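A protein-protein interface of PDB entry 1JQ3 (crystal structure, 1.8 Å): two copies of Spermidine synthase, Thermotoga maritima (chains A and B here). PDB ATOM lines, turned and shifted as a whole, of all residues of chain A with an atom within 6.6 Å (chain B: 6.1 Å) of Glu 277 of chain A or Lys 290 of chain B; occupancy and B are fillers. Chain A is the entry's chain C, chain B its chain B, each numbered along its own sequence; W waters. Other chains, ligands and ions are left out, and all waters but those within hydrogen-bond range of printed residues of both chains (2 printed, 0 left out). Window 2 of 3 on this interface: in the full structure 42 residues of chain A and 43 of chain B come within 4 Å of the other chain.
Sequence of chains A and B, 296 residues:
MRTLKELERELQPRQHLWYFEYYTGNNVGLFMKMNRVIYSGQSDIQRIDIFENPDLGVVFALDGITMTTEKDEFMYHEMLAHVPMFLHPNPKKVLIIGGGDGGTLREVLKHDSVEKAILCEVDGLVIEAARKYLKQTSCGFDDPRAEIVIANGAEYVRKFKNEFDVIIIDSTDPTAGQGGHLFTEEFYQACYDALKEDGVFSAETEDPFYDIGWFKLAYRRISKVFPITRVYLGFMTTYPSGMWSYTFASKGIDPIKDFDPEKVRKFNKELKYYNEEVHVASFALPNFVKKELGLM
NZ of Lys 290 of chain B lies within salt-bridge range of OE1 of Glu 277 of chain A, 2.9 Å away. The side-chain amide nitrogen (ND2) of Asn 275 of chain A sits at hydrogen-bond distance from the backbone carbonyl oxygen (O) of Leu 285 of chain B (3.0 Å). The side-chain amide nitrogen (ND2) of Asn 275 of chain A sits at hydrogen-bond distance from the side-chain amide oxygen (OD1) of Asn 287 of chain B (2.9 Å).
OG of Ser 282 of chain A lies close to O of Val 278 of chain A, at 3.4 Å. N of Val 278 of chain A lies within hydrogen-bond range of OD1 of Asn 275 of chain A (2.9 Å). OE2 of Glu 277 of chain A lies close to OD1 of Asn 275 of chain A, 3.1 Å away. The backbone carbonyl oxygen of Lys 290 of chain B is in hydrogen-bond range of the backbone NH of Leu 295 of chain B, 2.8 Å away.
Among the printed residues, merely in contact across the chains: Ala 281 of chain A with Ala 281 of chain B, Ala 281 of chain A with Ala 284 of chain B, Glu 277 of chain A with Ala 284 of chain B, Val 278 of chain A with Pro 286 of chain B, Val 278 of chain A with Leu 285 of chain B, Asn 275 of chain A with Pro 286 of chain B and Asn 275 of chain A with Lys 290 of chain B.
Glu 277 of chain A touches just these residues of chain B: Ala 284 and Lys 290. Lys 290 of chain B touches just these residues of chain A: Asn 275 and Glu 277. Of the printed residues of chain A, Asn 287 of chain B touches Asn 275 (2.9 Å). Of the printed residues of chain B, Ala 281 of chain A touches Ala 281 (3.5 Å) and Ala 284 (3.5 Å). Printed residues of chain A within 4 Å of Pro 286 of chain B: Asn 275 (3.9 Å) and Val 278 (3.7 Å). Of the printed residues of chain A, Ala 284 of chain B touches Glu 277 (3.5 Å) and Ala 281 (3.5 Å). Of the printed residues of chain A, Leu 285 of chain B touches Asn 275 (3.0 Å) and Val 278 (3.8 Å). The nearest residue of chain A that does not touch Lys 290 of chain B is Glu 276 of chain A (5.7 Å). The nearest printed residue of chain A that does not touch Ala 284 of chain B is Val 278 of chain A (4.1 Å).
Printed residues of chain B that touch a printed residue of chain A: Ala 281, Ala 284, Leu 285, Pro 286, Asn 287 and Lys 290. Hydrophobic or aromatic side chains of chain B that line the printed part of chain A: Ala 281 and Ala 284. Printed residues of chain A that touch a printed residue of chain B: Asn 275, Glu 277, Val 278 and Ala 281. Among the printed residues, 10 pairs touch across the chains. Among the printed residues, Asp or Glu carboxylates within 4 Å of a Lys or Arg side-chain nitrogen of the other chain: Glu 277 of chain A with Lys 290 of chain B.
Ala 281 of chain A touches its own counterpart, Ala 281 of chain B. Position printed for both chains: 281.
Water W2 lies within hydrogen-bond range of OE2 of Glu 277 of chain A (2.7 Å), NZ of Lys 290 of chain B (3.0 Å) and OE1 of Glu 276 of chain A (3.2 Å). Water W1 lies within hydrogen-bond range of the side-chain carboxylate (OE1) of Glu 277 of chain A (2.9 Å) and the backbone NH (N) of Leu 285 of chain B (3.0 Å).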
ATOM      1  N   PHE A 259       7.727   0.046   9.888  1.00  0.00           N
ATOM      2  CA  PHE A 259       8.467  -0.894  10.727  1.00  0.00           C
ATOM      3  C   PHE A 259       8.748  -2.188   9.968  1.00  0.00           C
ATOM      4  O   PHE A 259       7.828  -2.840   9.483  1.00  0.00           O
ATOM      5  CB  PHE A 259       7.674  -1.243  11.996  1.00  0.00           C
ATOM      6  CG  PHE A 259       8.394  -2.218  12.907  1.00  0.00           C
ATOM      7  CD1 PHE A 259       9.648  -1.903  13.423  1.00  0.00           C
ATOM      8  CD2 PHE A 259       7.809  -3.431  13.265  1.00  0.00           C
ATOM      9  CE1 PHE A 259      10.313  -2.773  14.283  1.00  0.00           C
ATOM     10  CE2 PHE A 259       8.466  -4.314  14.128  1.00  0.00           C
ATOM     11  CZ  PHE A 259       9.719  -3.982  14.638  1.00  0.00           C
ATOM     12  N   ARG A 265      14.670  -9.036  13.910  1.00  0.00           N
ATOM     13  CA  ARG A 265      14.922 -10.478  13.919  1.00  0.00           C
ATOM     14  C   ARG A 265      16.364 -10.831  13.595  1.00  0.00           C
ATOM     15  O   ARG A 265      16.919 -11.766  14.168  1.00  0.00           O
ATOM     16  CB  ARG A 265      13.998 -11.211  12.942  1.00  0.00           C
ATOM     17  CG  ARG A 265      12.645 -11.552  13.539  1.00  0.00           C
ATOM     18  CD  ARG A 265      11.815 -12.459  12.633  1.00  0.00           C
ATOM     19  NE  ARG A 265      11.368 -11.779  11.419  1.00  0.00           N
ATOM     20  CZ  ARG A 265      10.187 -11.181  11.282  1.00  0.00           C
ATOM     21  NH1 ARG A 265       9.316 -11.172  12.287  1.00  0.00           N
ATOM     22  NH2 ARG A 265       9.879 -10.585  10.139  1.00  0.00           N
ATOM     23  N   ASN A 275      11.658  -6.470  21.107  1.00  0.00           N
ATOM     24  CA  ASN A 275      11.558  -7.458  20.021  1.00  0.00           C
ATOM     25  C   ASN A 275      10.464  -6.986  19.051  1.00  0.00           C
ATOM     26  O   ASN A 275       9.787  -5.989  19.319  1.00  0.00           O
ATOM     27  CB  ASN A 275      11.319  -8.892  20.542  1.00  0.00           C
ATOM     28  CG  ASN A 275      10.009  -9.054  21.286  1.00  0.00           C
ATOM     29  OD1 ASN A 275       8.954  -8.637  20.811  1.00  0.00           O
ATOM     30  ND2 ASN A 275      10.070  -9.688  22.459  1.00  0.00           N
ATOM     31  N   GLU A 276      10.323  -7.658  17.910  1.00  0.00           N
ATOM     32  CA  GLU A 276       9.338  -7.253  16.894  1.00  0.00           C
ATOM     33  C   GLU A 276       7.891  -7.136  17.377  1.00  0.00           C
ATOM     34  O   GLU A 276       7.194  -6.198  16.981  1.00  0.00           O
ATOM     35  CB  GLU A 276       9.348  -8.188  15.665  1.00  0.00           C
ATOM     36  CG  GLU A 276      10.666  -8.820  15.302  1.00  0.00           C
ATOM     37  CD  GLU A 276      10.943 -10.059  16.120  1.00  0.00           C
ATOM     38  OE1 GLU A 276      10.418 -11.143  15.777  1.00  0.00           O
ATOM     39  OE2 GLU A 276      11.673  -9.941  17.113  1.00  0.00           O
ATOM     40  N   GLU A 277       7.417  -8.107  18.164  1.00  0.00           N
ATOM     41  CA  GLU A 277       6.027  -8.089  18.657  1.00  0.00           C
ATOM     42  C   GLU A 277       5.835  -6.945  19.640  1.00  0.00           C
ATOM     43  O   GLU A 277       4.777  -6.325  19.697  1.00  0.00           O
ATOM     44  CB  GLU A 277       5.647  -9.377  19.405  1.00  0.00           C
ATOM     45  CG  GLU A 277       6.141 -10.677  18.821  1.00  0.00           C
ATOM     46  CD  GLU A 277       7.482 -11.085  19.398  1.00  0.00           C
ATOM     47  OE1 GLU A 277       7.531 -11.618  20.538  1.00  0.00           O
ATOM     48  OE2 GLU A 277       8.484 -10.864  18.705  1.00  0.00           O
ATOM     49  N   VAL A 278       6.835  -6.744  20.481  1.00  0.00           N
ATOM     50  CA  VAL A 278       6.771  -5.679  21.483  1.00  0.00           C
ATOM     51  C   VAL A 278       6.783  -4.300  20.824  1.00  0.00           C
ATOM     52  O   VAL A 278       6.101  -3.373  21.294  1.00  0.00           O
ATOM     53  CB  VAL A 278       7.898  -5.856  22.520  1.00  0.00           C
ATOM     54  CG1 VAL A 278       8.117  -4.587  23.334  1.00  0.00           C
ATOM     55  CG2 VAL A 278       7.538  -7.041  23.433  1.00  0.00           C
ATOM     56  N   HIS A 279       7.531  -4.170  19.731  1.00  0.00           N
ATOM     57  CA  HIS A 279       7.583  -2.885  19.011  1.00  0.00           C
ATOM     58  C   HIS A 279       6.165  -2.468  18.634  1.00  0.00           C
ATOM     59  O   HIS A 279       5.703  -1.379  18.966  1.00  0.00           O
ATOM     60  CB  HIS A 279       8.418  -2.981  17.726  1.00  0.00           C
ATOM     61  CG  HIS A 279       8.535  -1.678  16.998  1.00  0.00           C
ATOM     62  ND1 HIS A 279       7.523  -1.170  16.206  1.00  0.00           N
ATOM     63  CD2 HIS A 279       9.528  -0.759  16.973  1.00  0.00           C
ATOM     64  CE1 HIS A 279       7.893   0.003  15.724  1.00  0.00           C
ATOM     65  NE2 HIS A 279       9.105   0.276  16.175  1.00  0.00           N
ATOM     66  N   VAL A 280       5.481  -3.348  17.912  1.00  0.00           N
ATOM     67  CA  VAL A 280       4.121  -3.084  17.464  1.00  0.00           C
ATOM     68  C   VAL A 280       3.134  -2.926  18.625  1.00  0.00           C
ATOM     69  O   VAL A 280       2.337  -1.988  18.655  1.00  0.00           O
ATOM     70  CB  VAL A 280       3.669  -4.192  16.502  1.00  0.00           C
ATOM     71  CG1 VAL A 280       2.206  -4.027  16.120  1.00  0.00           C
ATOM     72  CG2 VAL A 280       4.575  -4.166  15.250  1.00  0.00           C
ATOM     73  N   ALA A 281       3.237  -3.824  19.596  1.00  0.00           N
ATOM     74  CA  ALA A 281       2.366  -3.837  20.761  1.00  0.00           C
ATOM     75  C   ALA A 281       2.444  -2.588  21.633  1.00  0.00           C
ATOM     76  O   ALA A 281       1.423  -2.150  22.192  1.00  0.00           O
ATOM     77  CB  ALA A 281       2.660  -5.052  21.594  1.00  0.00           C
ATOM     78  N   SER A 282       3.639  -2.009  21.733  1.00  0.00           N
ATOM     79  CA  SER A 282       3.833  -0.828  22.580  1.00  0.00           C
ATOM     80  C   SER A 282       3.011   0.369  22.119  1.00  0.00           C
ATOM     81  O   SER A 282       2.751   1.282  22.916  1.00  0.00           O
ATOM     82  CB  SER A 282       5.321  -0.458  22.691  1.00  0.00           C
ATOM     83  OG  SER A 282       5.829  -0.006  21.453  1.00  0.00           O
ATOM     84  N   ALA B 281      -2.203  -6.776  21.670  1.00  0.00           N
ATOM     85  CA  ALA B 281      -0.889  -6.320  22.155  1.00  0.00           C
ATOM     86  C   ALA B 281      -0.459  -6.934  23.484  1.00  0.00           C
ATOM     87  O   ALA B 281       0.740  -7.129  23.714  1.00  0.00           O
ATOM     88  CB  ALA B 281      -0.848  -4.793  22.268  1.00  0.00           C
ATOM     89  N   ALA B 284       2.014  -9.859  23.499  1.00  0.00           N
ATOM     90  CA  ALA B 284       3.404  -9.667  23.068  1.00  0.00           C
ATOM     91  C   ALA B 284       4.284  -9.632  24.322  1.00  0.00           C
ATOM     92  O   ALA B 284       4.161  -8.728  25.160  1.00  0.00           O
ATOM     93  CB  ALA B 284       3.547  -8.369  22.271  1.00  0.00           C
ATOM     94  N   LEU B 285       5.157 -10.629  24.464  1.00  0.00           N
ATOM     95  CA  LEU B 285       6.003 -10.714  25.645  1.00  0.00           C
ATOM     96  C   LEU B 285       7.425 -10.243  25.414  1.00  0.00           C
ATOM     97  O   LEU B 285       8.065 -10.634  24.424  1.00  0.00           O
ATOM     98  CB  LEU B 285       6.067 -12.162  26.143  1.00  0.00           C
ATOM     99  CG  LEU B 285       4.762 -12.952  26.320  1.00  0.00           C
ATOM    100  CD1 LEU B 285       5.102 -14.335  26.882  1.00  0.00           C
ATOM    101  CD2 LEU B 285       3.816 -12.211  27.272  1.00  0.00           C
ATOM    102  N   PRO B 286       7.938  -9.386  26.306  1.00  0.00           N
ATOM    103  CA  PRO B 286       9.312  -8.884  26.189  1.00  0.00           C
ATOM    104  C   PRO B 286      10.277 -10.094  26.286  1.00  0.00           C
ATOM    105  O   PRO B 286       9.933 -11.137  26.880  1.00  0.00           O
ATOM    106  CB  PRO B 286       9.442  -7.974  27.408  1.00  0.00           C
ATOM    107  CG  PRO B 286       8.033  -7.458  27.597  1.00  0.00           C
ATOM    108  CD  PRO B 286       7.210  -8.707  27.400  1.00  0.00           C
ATOM    109  N   ASN B 287      11.469  -9.959  25.706  1.00  0.00           N
ATOM    110  CA  ASN B 287      12.442 -11.047  25.717  1.00  0.00           C
ATOM    111  C   ASN B 287      12.723 -11.707  27.075  1.00  0.00           C
ATOM    112  O   ASN B 287      12.710 -12.934  27.166  1.00  0.00           O
ATOM    113  CB  ASN B 287      13.765 -10.598  25.068  1.00  0.00           C
ATOM    114  CG  ASN B 287      13.696 -10.546  23.542  1.00  0.00           C
ATOM    115  OD1 ASN B 287      12.680 -10.867  22.930  1.00  0.00           O
ATOM    116  ND2 ASN B 287      14.800 -10.136  22.926  1.00  0.00           N
ATOM    117  N   PHE B 288      12.946 -10.915  28.130  1.00  0.00           N
ATOM    118  CA  PHE B 288      13.247 -11.498  29.443  1.00  0.00           C
ATOM    119  C   PHE B 288      12.126 -12.401  29.963  1.00  0.00           C
ATOM    120  O   PHE B 288      12.389 -13.381  30.657  1.00  0.00           O
ATOM    121  CB  PHE B 288      13.634 -10.433  30.490  1.00  0.00           C
ATOM    122  CG  PHE B 288      12.462  -9.697  31.098  1.00  0.00           C
ATOM    123  CD1 PHE B 288      11.892  -8.599  30.454  1.00  0.00           C
ATOM    124  CD2 PHE B 288      11.959 -10.073  32.347  1.00  0.00           C
ATOM    125  CE1 PHE B 288      10.832  -7.882  31.052  1.00  0.00           C
ATOM    126  CE2 PHE B 288      10.900  -9.360  32.949  1.00  0.00           C
ATOM    127  CZ  PHE B 288      10.344  -8.269  32.298  1.00  0.00           C
ATOM    128  N   VAL B 289      10.889 -12.098  29.574  1.00  0.00           N
ATOM    129  CA  VAL B 289       9.735 -12.903  29.997  1.00  0.00           C
ATOM    130  C   VAL B 289       9.731 -14.195  29.191  1.00  0.00           C
ATOM    131  O   VAL B 289       9.568 -15.283  29.753  1.00  0.00           O
ATOM    132  CB  VAL B 289       8.388 -12.163  29.788  1.00  0.00           C
ATOM    133  CG1 VAL B 289       7.222 -13.098  30.130  1.00  0.00           C
ATOM    134  CG2 VAL B 289       8.317 -10.922  30.675  1.00  0.00           C
ATOM    135  N   LYS B 290       9.952 -14.073  27.888  1.00  0.00           N
ATOM    136  CA  LYS B 290       9.993 -15.238  27.002  1.00  0.00           C
ATOM    137  C   LYS B 290      11.084 -16.208  27.480  1.00  0.00           C
ATOM    138  O   LYS B 290      10.866 -17.431  27.571  1.00  0.00           O
ATOM    139  CB  LYS B 290      10.256 -14.801  25.551  1.00  0.00           C
ATOM    140  CG  LYS B 290       9.041 -14.147  24.889  1.00  0.00           C
ATOM    141  CD  LYS B 290       9.389 -13.330  23.640  1.00  0.00           C
ATOM    142  CE  LYS B 290       9.712 -14.190  22.453  1.00  0.00           C
ATOM    143  NZ  LYS B 290       9.735 -13.390  21.189  1.00  0.00           N
ATOM    144  N   LYS B 291      12.224 -15.647  27.865  1.00  0.00           N
ATOM    145  CA  LYS B 291      13.345 -16.451  28.337  1.00  0.00           C
ATOM    146  C   LYS B 291      12.966 -17.186  29.629  1.00  0.00           C
ATOM    147  O   LYS B 291      13.274 -18.378  29.784  1.00  0.00           O
ATOM    148  CB  LYS B 291      14.599 -15.575  28.521  1.00  0.00           C
ATOM    149  CG  LYS B 291      15.830 -16.343  29.020  1.00  0.00           C
ATOM    150  CD  LYS B 291      17.142 -15.540  28.922  1.00  0.00           C
ATOM    151  CE  LYS B 291      17.675 -15.489  27.496  1.00  0.00           C
ATOM    152  NZ  LYS B 291      19.043 -14.879  27.385  1.00  0.00           N
ATOM    153  N   GLU B 292      12.272 -16.497  30.535  1.00  0.00           N
ATOM    154  CA  GLU B 292      11.859 -17.120  31.786  1.00  0.00           C
ATOM    155  C   GLU B 292      10.884 -18.283  31.594  1.00  0.00           C
ATOM    156  O   GLU B 292      10.902 -19.242  32.369  1.00  0.00           O
ATOM    157  CB  GLU B 292      11.276 -16.091  32.763  1.00  0.00           C
ATOM    158  CG  GLU B 292      12.331 -15.242  33.498  1.00  0.00           C
ATOM    159  CD  GLU B 292      13.282 -16.061  34.397  1.00  0.00           C
ATOM    160  OE1 GLU B 292      13.134 -17.302  34.510  1.00  0.00           O
ATOM    161  OE2 GLU B 292      14.197 -15.452  34.995  1.00  0.00           O
ATOM    162  N   LEU B 293      10.066 -18.210  30.544  1.00  0.00           N
ATOM    163  CA  LEU B 293       9.081 -19.253  30.258  1.00  0.00           C
ATOM    164  C   LEU B 293       9.611 -20.298  29.288  1.00  0.00           C
ATOM    165  O   LEU B 293       8.913 -21.262  28.969  1.00  0.00           O
ATOM    166  CB  LEU B 293       7.815 -18.630  29.669  1.00  0.00           C
ATOM    167  CG  LEU B 293       7.095 -17.664  30.601  1.00  0.00           C
ATOM    168  CD1 LEU B 293       5.963 -16.993  29.856  1.00  0.00           C
ATOM    169  CD2 LEU B 293       6.581 -18.422  31.808  1.00  0.00           C
ATOM    170  N   GLY B 294      10.823 -20.068  28.786  1.00  0.00           N
ATOM    171  CA  GLY B 294      11.436 -20.982  27.839  1.00  0.00           C
ATOM    172  C   GLY B 294      10.880 -20.864  26.431  1.00  0.00           C
ATOM    173  O   GLY B 294      10.972 -21.808  25.641  1.00  0.00           O
ATOM    174  N   LEU B 295      10.308 -19.705  26.109  1.00  0.00           N
ATOM    175  CA  LEU B 295       9.738 -19.470  24.786  1.00  0.00           C
ATOM    176  C   LEU B 295      10.755 -18.787  23.882  1.00  0.00           C
ATOM    177  O   LEU B 295      10.391 -18.028  22.985  1.00  0.00           O
ATOM    178  CB  LEU B 295       8.463 -18.628  24.893  1.00  0.00           C
ATOM    179  CG  LEU B 295       7.422 -19.127  25.898  1.00  0.00           C
ATOM    180  CD1 LEU B 295       6.200 -18.223  25.856  1.00  0.00           C
ATOM    181  CD2 LEU B 295       7.044 -20.572  25.582  1.00  0.00           C
ATOM    182  N   MET B 296      12.029 -19.090  24.128  1.00  0.00           N
ATOM    183  CA  MET B 296      13.165 -18.559  23.367  1.00  0.00           C
ATOM    184  C   MET B 296      13.326 -17.056  23.553  1.00  0.00           C
ATOM    185  O   MET B 296      12.780 -16.292  22.722  1.00  0.00           O
ATOM    186  CB  MET B 296      13.041 -18.921  21.874  1.00  0.00           C
ATOM    187  OXT MET B 296      13.990 -16.664  24.539  1.00  0.00           O
HETATM  188  O   HOH W   1       5.637 -12.746  22.430  1.00  0.00           O
HETATM  189  O   HOH W   2      10.009 -13.064  18.242  1.00  0.00           O
